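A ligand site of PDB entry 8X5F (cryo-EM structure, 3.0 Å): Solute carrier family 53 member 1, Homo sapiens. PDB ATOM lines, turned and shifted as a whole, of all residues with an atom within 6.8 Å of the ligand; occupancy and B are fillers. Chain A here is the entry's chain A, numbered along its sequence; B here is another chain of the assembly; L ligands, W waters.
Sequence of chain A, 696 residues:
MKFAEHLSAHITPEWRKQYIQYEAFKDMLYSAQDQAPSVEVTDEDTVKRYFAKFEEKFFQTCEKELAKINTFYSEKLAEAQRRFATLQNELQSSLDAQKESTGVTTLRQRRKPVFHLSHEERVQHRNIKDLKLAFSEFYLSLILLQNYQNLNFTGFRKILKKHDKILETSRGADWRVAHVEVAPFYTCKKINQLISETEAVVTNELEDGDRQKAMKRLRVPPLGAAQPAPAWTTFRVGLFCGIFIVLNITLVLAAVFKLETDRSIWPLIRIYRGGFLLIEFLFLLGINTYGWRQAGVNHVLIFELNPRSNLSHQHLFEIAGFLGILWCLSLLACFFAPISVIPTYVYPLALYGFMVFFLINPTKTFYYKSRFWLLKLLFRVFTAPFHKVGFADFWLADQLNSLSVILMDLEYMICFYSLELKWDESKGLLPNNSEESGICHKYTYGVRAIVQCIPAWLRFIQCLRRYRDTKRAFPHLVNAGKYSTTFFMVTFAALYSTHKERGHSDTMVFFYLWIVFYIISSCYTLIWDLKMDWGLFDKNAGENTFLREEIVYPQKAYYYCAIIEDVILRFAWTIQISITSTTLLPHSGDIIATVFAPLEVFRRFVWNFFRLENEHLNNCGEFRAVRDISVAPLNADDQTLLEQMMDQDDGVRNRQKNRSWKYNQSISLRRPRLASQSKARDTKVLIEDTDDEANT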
ATOM      1  N   MET A   1     -17.188  10.031 -15.310  1.00  0.00           N
ATOM      2  CA  MET A   1     -17.361   9.935 -13.860  1.00  0.00           C
ATOM      3  C   MET A   1     -18.088   8.654 -13.482  1.00  0.00           C
ATOM      4  O   MET A   1     -19.184   8.702 -12.917  1.00  0.00           O
ATOM      5  CB  MET A   1     -18.127  11.146 -13.331  1.00  0.00           C
ATOM      6  N   LYS A   2     -17.492   7.494 -13.801  1.00  0.00           N
ATOM      7  CA  LYS A   2     -18.123   6.220 -13.548  1.00  0.00           C
ATOM      8  C   LYS A   2     -17.524   5.592 -12.307  1.00  0.00           C
ATOM      9  O   LYS A   2     -18.248   5.366 -11.322  1.00  0.00           O
ATOM     10  CB  LYS A   2     -18.002   5.306 -14.779  1.00  0.00           C
ATOM     11  CG  LYS A   2     -18.711   5.818 -16.016  1.00  0.00           C
ATOM     12  CD  LYS A   2     -20.209   5.703 -15.893  1.00  0.00           C
ATOM     13  CE  LYS A   2     -20.888   6.192 -17.155  1.00  0.00           C
ATOM     14  NZ  LYS A   2     -20.581   5.316 -18.313  1.00  0.00           N
ATOM     15  N   PHE A   3     -16.212   5.308 -12.278  1.00  0.00           N
ATOM     16  CA  PHE A   3     -15.722   4.376 -11.259  1.00  0.00           C
ATOM     17  C   PHE A   3     -14.910   5.065 -10.184  1.00  0.00           C
ATOM     18  O   PHE A   3     -14.790   4.543  -9.071  1.00  0.00           O
ATOM     19  CB  PHE A   3     -14.895   3.266 -11.895  1.00  0.00           C
ATOM     20  CG  PHE A   3     -14.550   2.167 -10.936  1.00  0.00           C
ATOM     21  CD1 PHE A   3     -15.539   1.337 -10.433  1.00  0.00           C
ATOM     22  CD2 PHE A   3     -13.261   1.984 -10.503  1.00  0.00           C
ATOM     23  CE1 PHE A   3     -15.232   0.333  -9.541  1.00  0.00           C
ATOM     24  CE2 PHE A   3     -12.941   0.985  -9.608  1.00  0.00           C
ATOM     25  CZ  PHE A   3     -13.936   0.161  -9.127  1.00  0.00           C
ATOM     26  N   ALA A   4     -14.315   6.220 -10.477  1.00  0.00           N
ATOM     27  CA  ALA A   4     -13.579   6.921  -9.431  1.00  0.00           C
ATOM     28  C   ALA A   4     -14.512   7.326  -8.290  1.00  0.00           C
ATOM     29  O   ALA A   4     -14.212   7.058  -7.115  1.00  0.00           O
ATOM     30  CB  ALA A   4     -12.871   8.149 -10.012  1.00  0.00           C
ATOM     31  N   TYR A  22      -6.685   3.835  -7.560  1.00  0.00           N
ATOM     32  CA  TYR A  22      -7.162   4.104  -8.913  1.00  0.00           C
ATOM     33  C   TYR A  22      -6.679   5.462  -9.414  1.00  0.00           C
ATOM     34  O   TYR A  22      -6.251   5.590 -10.567  1.00  0.00           O
ATOM     35  CB  TYR A  22      -8.683   4.024  -8.924  1.00  0.00           C
ATOM     36  CG  TYR A  22      -9.305   3.815 -10.277  1.00  0.00           C
ATOM     37  CD1 TYR A  22      -9.292   2.562 -10.881  1.00  0.00           C
ATOM     38  CD2 TYR A  22      -9.931   4.849 -10.943  1.00  0.00           C
ATOM     39  CE1 TYR A  22      -9.865   2.362 -12.119  1.00  0.00           C
ATOM     40  CE2 TYR A  22     -10.509   4.657 -12.178  1.00  0.00           C
ATOM     41  CZ  TYR A  22     -10.470   3.409 -12.763  1.00  0.00           C
ATOM     42  OH  TYR A  22     -11.048   3.212 -13.985  1.00  0.00           O
ATOM     43  N   LYS A  26      -4.306   6.425 -12.932  1.00  0.00           N
ATOM     44  CA  LYS A  26      -4.885   7.241 -13.977  1.00  0.00           C
ATOM     45  C   LYS A  26      -3.988   8.401 -14.239  1.00  0.00           C
ATOM     46  O   LYS A  26      -3.665   8.686 -15.378  1.00  0.00           O
ATOM     47  CB  LYS A  26      -6.242   7.772 -13.552  1.00  0.00           C
ATOM     48  CG  LYS A  26      -7.394   6.811 -13.677  1.00  0.00           C
ATOM     49  CD  LYS A  26      -8.666   7.465 -13.161  1.00  0.00           C
ATOM     50  CE  LYS A  26      -8.918   8.797 -13.838  1.00  0.00           C
ATOM     51  NZ  LYS A  26     -10.120   9.470 -13.287  1.00  0.00           N
ATOM     52  N   TYR A  30      -2.054   9.369 -17.719  1.00  0.00           N
ATOM     53  CA  TYR A  30      -2.360  10.610 -18.410  1.00  0.00           C
ATOM     54  C   TYR A  30      -1.102  11.403 -18.629  1.00  0.00           C
ATOM     55  O   TYR A  30      -0.893  11.909 -19.719  1.00  0.00           O
ATOM     56  CB  TYR A  30      -3.389  11.430 -17.643  1.00  0.00           C
ATOM     57  CG  TYR A  30      -4.775  10.825 -17.670  1.00  0.00           C
ATOM     58  CD1 TYR A  30      -5.218  10.101 -18.768  1.00  0.00           C
ATOM     59  CD2 TYR A  30      -5.644  10.995 -16.603  1.00  0.00           C
ATOM     60  CE1 TYR A  30      -6.482   9.554 -18.787  1.00  0.00           C
ATOM     61  CE2 TYR A  30      -6.918  10.450 -16.613  1.00  0.00           C
ATOM     62  CZ  TYR A  30      -7.325   9.734 -17.714  1.00  0.00           C
ATOM     63  OH  TYR A  30      -8.594   9.186 -17.740  1.00  0.00           O
ATOM     64  N   ARG A 157      -9.777  -4.727 -13.028  1.00  0.00           N
ATOM     65  CA  ARG A 157     -10.243  -4.951 -14.389  1.00  0.00           C
ATOM     66  C   ARG A 157     -10.404  -3.644 -15.152  1.00  0.00           C
ATOM     67  O   ARG A 157      -9.934  -3.515 -16.286  1.00  0.00           O
ATOM     68  CB  ARG A 157     -11.559  -5.724 -14.365  1.00  0.00           C
ATOM     69  CG  ARG A 157     -12.082  -6.097 -15.727  1.00  0.00           C
ATOM     70  CD  ARG A 157     -13.466  -6.713 -15.642  1.00  0.00           C
ATOM     71  NE  ARG A 157     -14.513  -5.700 -15.613  1.00  0.00           N
ATOM     72  CZ  ARG A 157     -14.876  -4.959 -16.652  1.00  0.00           C
ATOM     73  NH1 ARG A 157     -14.302  -5.107 -17.830  1.00  0.00           N
ATOM     74  NH2 ARG A 157     -15.841  -4.065 -16.502  1.00  0.00           N
ATOM     75  N   LYS A 158     -11.029  -2.645 -14.527  1.00  0.00           N
ATOM     76  CA  LYS A 158     -11.301  -1.405 -15.232  1.00  0.00           C
ATOM     77  C   LYS A 158     -10.013  -0.631 -15.513  1.00  0.00           C
ATOM     78  O   LYS A 158      -9.856  -0.056 -16.597  1.00  0.00           O
ATOM     79  CB  LYS A 158     -12.301  -0.560 -14.460  1.00  0.00           C
ATOM     80  CG  LYS A 158     -13.692  -1.163 -14.471  1.00  0.00           C
ATOM     81  CD  LYS A 158     -14.736  -0.210 -13.940  1.00  0.00           C
ATOM     82  CE  LYS A 158     -16.131  -0.739 -14.236  1.00  0.00           C
ATOM     83  NZ  LYS A 158     -17.202   0.221 -13.836  1.00  0.00           N
ATOM     84  N   LYS A 161      -8.218  -2.297 -18.416  1.00  0.00           N
ATOM     85  CA  LYS A 161      -8.883  -1.983 -19.671  1.00  0.00           C
ATOM     86  C   LYS A 161      -8.547  -0.573 -20.131  1.00  0.00           C
ATOM     87  O   LYS A 161      -8.295  -0.336 -21.320  1.00  0.00           O
ATOM     88  CB  LYS A 161     -10.395  -2.173 -19.529  1.00  0.00           C
ATOM     89  CG  LYS A 161     -11.184  -1.947 -20.807  1.00  0.00           C
ATOM     90  CD  LYS A 161     -11.926  -0.629 -20.773  1.00  0.00           C
ATOM     91  CE  LYS A 161     -13.124  -0.707 -19.842  1.00  0.00           C
ATOM     92  NZ  LYS A 161     -13.900   0.560 -19.809  1.00  0.00           N
ATOM     93  N   LYS A 162      -8.518   0.398 -19.218  1.00  0.00           N
ATOM     94  CA  LYS A 162      -8.137   1.774 -19.575  1.00  0.00           C
ATOM     95  C   LYS A 162      -6.696   1.798 -20.077  1.00  0.00           C
ATOM     96  O   LYS A 162      -6.407   2.483 -21.043  1.00  0.00           O
ATOM     97  CB  LYS A 162      -8.294   2.726 -18.391  1.00  0.00           C
ATOM     98  CG  LYS A 162      -8.255   4.194 -18.744  1.00  0.00           C
ATOM     99  CD  LYS A 162      -8.085   5.055 -17.501  1.00  0.00           C
ATOM    100  CE  LYS A 162      -9.011   4.604 -16.394  1.00  0.00           C
ATOM    101  NZ  LYS A 162     -10.456   4.837 -16.678  1.00  0.00           N
ATOM    102  N   LYS A 165      -6.618   0.606 -23.547  1.00  0.00           N
ATOM    103  CA  LYS A 165      -7.187   1.617 -24.424  1.00  0.00           C
ATOM    104  C   LYS A 165      -6.183   2.730 -24.734  1.00  0.00           C
ATOM    105  O   LYS A 165      -6.013   3.115 -25.889  1.00  0.00           O
ATOM    106  CB  LYS A 165      -8.455   2.207 -23.812  1.00  0.00           C
ATOM    107  CG  LYS A 165      -9.087   3.307 -24.636  1.00  0.00           C
ATOM    108  CD  LYS A 165     -10.384   3.773 -24.020  1.00  0.00           C
ATOM    109  CE  LYS A 165     -10.982   4.921 -24.805  1.00  0.00           C
ATOM    110  NZ  LYS A 165     -12.278   5.374 -24.242  1.00  0.00           N
ATOM    111  N   ILE A 166      -5.512   3.247 -23.697  1.00  0.00           N
ATOM    112  CA  ILE A 166      -4.687   4.442 -23.876  1.00  0.00           C
ATOM    113  C   ILE A 166      -3.461   4.154 -24.732  1.00  0.00           C
ATOM    114  O   ILE A 166      -3.163   4.882 -25.678  1.00  0.00           O
ATOM    115  CB  ILE A 166      -4.303   5.043 -22.509  1.00  0.00           C
ATOM    116  CG1 ILE A 166      -5.526   5.667 -21.841  1.00  0.00           C
ATOM    117  CG2 ILE A 166      -3.204   6.067 -22.669  1.00  0.00           C
ATOM    118  CD1 ILE A 166      -5.211   6.389 -20.555  1.00  0.00           C
ATOM    119  N   GLU B 199     -22.325   2.002 -33.640  1.00  0.00           N
ATOM    120  CA  GLU B 199     -21.450   3.014 -33.067  1.00  0.00           C
ATOM    121  C   GLU B 199     -20.162   3.161 -33.862  1.00  0.00           C
ATOM    122  O   GLU B 199     -19.611   4.256 -33.959  1.00  0.00           O
ATOM    123  CB  GLU B 199     -21.165   2.691 -31.591  1.00  0.00           C
ATOM    124  CG  GLU B 199     -20.381   1.436 -31.338  1.00  0.00           C
ATOM    125  CD  GLU B 199     -20.204   1.163 -29.852  1.00  0.00           C
ATOM    126  OE1 GLU B 199     -20.736   1.960 -29.043  1.00  0.00           O
ATOM    127  OE2 GLU B 199     -19.554   0.166 -29.494  1.00  0.00           O
ATOM    128  N   ARG B 211     -14.518   9.182 -31.041  1.00  0.00           N
ATOM    129  CA  ARG B 211     -15.441   8.260 -30.391  1.00  0.00           C
ATOM    130  C   ARG B 211     -16.161   8.911 -29.214  1.00  0.00           C
ATOM    131  O   ARG B 211     -17.299   8.545 -28.902  1.00  0.00           O
ATOM    132  CB  ARG B 211     -14.693   7.011 -29.919  1.00  0.00           C
ATOM    133  CG  ARG B 211     -15.580   5.992 -29.226  1.00  0.00           C
ATOM    134  CD  ARG B 211     -14.829   4.724 -28.871  1.00  0.00           C
ATOM    135  NE  ARG B 211     -15.660   3.820 -28.076  1.00  0.00           N
ATOM    136  CZ  ARG B 211     -16.507   2.945 -28.600  1.00  0.00           C
ATOM    137  NH1 ARG B 211     -16.683   2.838 -29.902  1.00  0.00           N
ATOM    138  NH2 ARG B 211     -17.210   2.156 -27.786  1.00  0.00           N
ATOM    139  N   GLN B 212     -15.507   9.852 -28.536  1.00  0.00           N
ATOM    140  CA  GLN B 212     -16.103  10.438 -27.344  1.00  0.00           C
ATOM    141  C   GLN B 212     -17.384  11.201 -27.666  1.00  0.00           C
ATOM    142  O   GLN B 212     -18.396  11.043 -26.973  1.00  0.00           O
ATOM    143  CB  GLN B 212     -15.090  11.337 -26.631  1.00  0.00           C
ATOM    144  CG  GLN B 212     -15.588  11.889 -25.302  1.00  0.00           C
ATOM    145  CD  GLN B 212     -14.515  12.630 -24.542  1.00  0.00           C
ATOM    146  OE1 GLN B 212     -13.402  12.809 -25.033  1.00  0.00           O
ATOM    147  NE2 GLN B 212     -14.845  13.066 -23.337  1.00  0.00           N
ATOM    148  N   MET B 215     -20.183   8.689 -28.613  1.00  0.00           N
ATOM    149  CA  MET B 215     -20.709   7.926 -27.491  1.00  0.00           C
ATOM    150  C   MET B 215     -21.473   8.825 -26.521  1.00  0.00           C
ATOM    151  O   MET B 215     -22.378   8.359 -25.825  1.00  0.00           O
ATOM    152  CB  MET B 215     -19.580   7.201 -26.770  1.00  0.00           C
ATOM    153  CG  MET B 215     -19.283   5.832 -27.360  1.00  0.00           C
ATOM    154  SD  MET B 215     -20.777   4.864 -27.613  1.00  0.00           S
ATOM    155  CE  MET B 215     -20.914   4.007 -26.050  1.00  0.00           C
ATOM    156  N   LYS B 216     -21.127  10.110 -26.462  1.00  0.00           N
ATOM    157  CA  LYS B 216     -21.927  11.049 -25.678  1.00  0.00           C
ATOM    158  C   LYS B 216     -23.326  11.187 -26.268  1.00  0.00           C
ATOM    159  O   LYS B 216     -24.308  11.361 -25.531  1.00  0.00           O
ATOM    160  CB  LYS B 216     -21.226  12.405 -25.625  1.00  0.00           C
ATOM    161  CG  LYS B 216     -21.943  13.423 -24.762  1.00  0.00           C
ATOM    162  CD  LYS B 216     -21.174  14.738 -24.702  1.00  0.00           C
ATOM    163  CE  LYS B 216     -21.847  15.719 -23.760  1.00  0.00           C
ATOM    164  NZ  LYS B 216     -23.171  16.175 -24.279  1.00  0.00           N
ATOM    165  N   ARG B 219     -25.199   7.331 -25.883  1.00  0.00           N
ATOM    166  CA  ARG B 219     -25.373   6.679 -24.586  1.00  0.00           C
ATOM    167  C   ARG B 219     -26.762   6.948 -24.010  1.00  0.00           C
ATOM    168  O   ARG B 219     -27.291   8.056 -24.101  1.00  0.00           O
ATOM    169  CB  ARG B 219     -24.302   7.145 -23.609  1.00  0.00           C
ATOM    170  CG  ARG B 219     -24.079   6.196 -22.446  1.00  0.00           C
ATOM    171  CD  ARG B 219     -22.784   6.532 -21.714  1.00  0.00           C
ATOM    172  NE  ARG B 219     -21.688   5.675 -22.128  1.00  0.00           N
ATOM    173  CZ  ARG B 219     -20.557   6.114 -22.671  1.00  0.00           C
ATOM    174  NH1 ARG B 219     -20.366   7.398 -22.923  1.00  0.00           N
ATOM    175  NH2 ARG B 219     -19.602   5.236 -22.977  1.00  0.00           N
HETATM  176  C1  LIG L   1     -16.522   3.802 -19.840  1.00  0.00           C
HETATM  177  C2  LIG L   1     -16.136   4.266 -21.261  1.00  0.00           C
HETATM  178  C3  LIG L   1     -15.608   5.696 -21.298  1.00  0.00           C
HETATM  179  C4  LIG L   1     -14.586   5.907 -20.207  1.00  0.00           C
HETATM  180  C5  LIG L   1     -15.336   5.870 -18.887  1.00  0.00           C
HETATM  181  C6  LIG L   1     -15.646   4.389 -18.731  1.00  0.00           C
HETATM  182  O1  LIG L   1     -16.449   2.402 -19.762  1.00  0.00           O
HETATM  183  P1  LIG L   1     -17.752   1.440 -20.112  1.00  0.00           P
HETATM  184  O2  LIG L   1     -17.700   1.011 -21.544  1.00  0.00           O
HETATM  185  O3  LIG L   1     -17.747   0.190 -19.276  1.00  0.00           O
HETATM  186  O4  LIG L   1     -19.017   2.208 -19.824  1.00  0.00           O
HETATM  187  O5  LIG L   1     -15.216   3.394 -21.869  1.00  0.00           O
HETATM  188  P2  LIG L   1     -15.463   2.972 -23.435  1.00  0.00           P
HETATM  189  O6  LIG L   1     -15.527   4.194 -24.303  1.00  0.00           O
HETATM  190  O7  LIG L   1     -14.344   2.097 -23.919  1.00  0.00           O
HETATM  191  O8  LIG L   1     -16.762   2.232 -23.575  1.00  0.00           O
HETATM  192  O9  LIG L   1     -14.985   5.940 -22.521  1.00  0.00           O
HETATM  193  P3  LIG L   1     -15.530   7.107 -23.537  1.00  0.00           P
HETATM  194  O10 LIG L   1     -16.545   6.527 -24.462  1.00  0.00           O
HETATM  195  O11 LIG L   1     -16.167   8.224 -22.757  1.00  0.00           O
HETATM  196  O12 LIG L   1     -14.362   7.645 -24.320  1.00  0.00           O
HETATM  197  O13 LIG L   1     -13.912   7.115 -20.394  1.00  0.00           O
HETATM  198  P4  LIG L   1     -12.266   7.112 -20.409  1.00  0.00           P
HETATM  199  O14 LIG L   1     -11.718   7.246 -21.795  1.00  0.00           O
HETATM  200  O15 LIG L   1     -11.754   8.260 -19.572  1.00  0.00           O
HETATM  201  O16 LIG L   1     -11.772   5.809 -19.856  1.00  0.00           O
HETATM  202  O17 LIG L   1     -14.466   6.290 -17.870  1.00  0.00           O
HETATM  203  P5  LIG L   1     -14.694   7.507 -16.770  1.00  0.00           P
HETATM  204  O18 LIG L   1     -16.150   7.703 -16.487  1.00  0.00           O
HETATM  205  O19 LIG L   1     -13.930   7.154 -15.504  1.00  0.00           O
HETATM  206  O20 LIG L   1     -14.149   8.794 -17.285  1.00  0.00           O
HETATM  207  O21 LIG L   1     -16.281   4.170 -17.497  1.00  0.00           O
HETATM  208  P6  LIG L   1     -15.594   3.118 -16.446  1.00  0.00           P
HETATM  209  O22 LIG L   1     -14.629   3.859 -15.589  1.00  0.00           O
HETATM  210  O23 LIG L   1     -16.652   2.524 -15.574  1.00  0.00           O
HETATM  211  O24 LIG L   1     -14.866   2.044 -17.194  1.00  0.00           O
HETATM  212  O   HOH W   1     -12.375   6.900 -13.645  1.00  0.00           O
HETATM  213  O   HOH W   2     -10.985   9.274 -17.229  1.00  0.00           O
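O24 of the ligand lies within salt-bridge range of NZ of Lys 161. N of Lys 2 is in hydrogen-bond range of O18 of the ligand. The side-chain amino group (NZ) of Lys 162 is in salt-bridge range of an oxygen (O16) of the ligand (3.6 Å). NZ of Lys 158 lies within salt-bridge range of O23 of the ligand (2.9 Å). The guanidinium group (NE) of Arg 211 of chain B lies within salt-bridge range of an oxygen (O6) of the ligand, at 3.8 Å. NH2 of Arg 219 of chain B is in salt-bridge range of O10 of the ligand (3.6 Å). NZ of Lys 165 lies within salt-bridge range of O12 of the ligand, at 3.1 Å. The backbone NH (N) of Met 1 lies within hydrogen-bond range of an oxygen (O18) of the ligand, at 2.8 Å. The side-chain amino group of Lys 2 is in salt-bridge range of an oxygen (O4) of the ligand (3.8 Å).
The side-chain amino group (NZ) of Lys 162 lies within hydrogen-bond range of the side-chain hydroxyl (OH) of Tyr 22.
Phe 3 touches the ligand (CB to O22, 3.8 Å). Tyr 22 touches the ligand. OH of Tyr 30 touches O15 of the ligand, 3.8 Å away. Met 215 of chain B touches the ligand. Hydrophobic or aromatic side chains within 4 Å of the ligand: Phe 3 and Met 215 of chain B. Within 4 Å of the ligand: Met 1, Lys 2, Phe 3, Tyr 22, Tyr 30, Lys 158, Lys 161, Lys 162, Lys 165, Arg 211 of chain B, Met 215 of chain B and Arg 219 of chain B.
Water W1 lies within hydrogen-bond range of an oxygen (O19) of the ligand and the side-chain amino group of Lys 26. Water W2 lies within hydrogen-bond range of OH of Tyr 30 (2.4 Å) and O15 of the ligand (2.7 Å).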
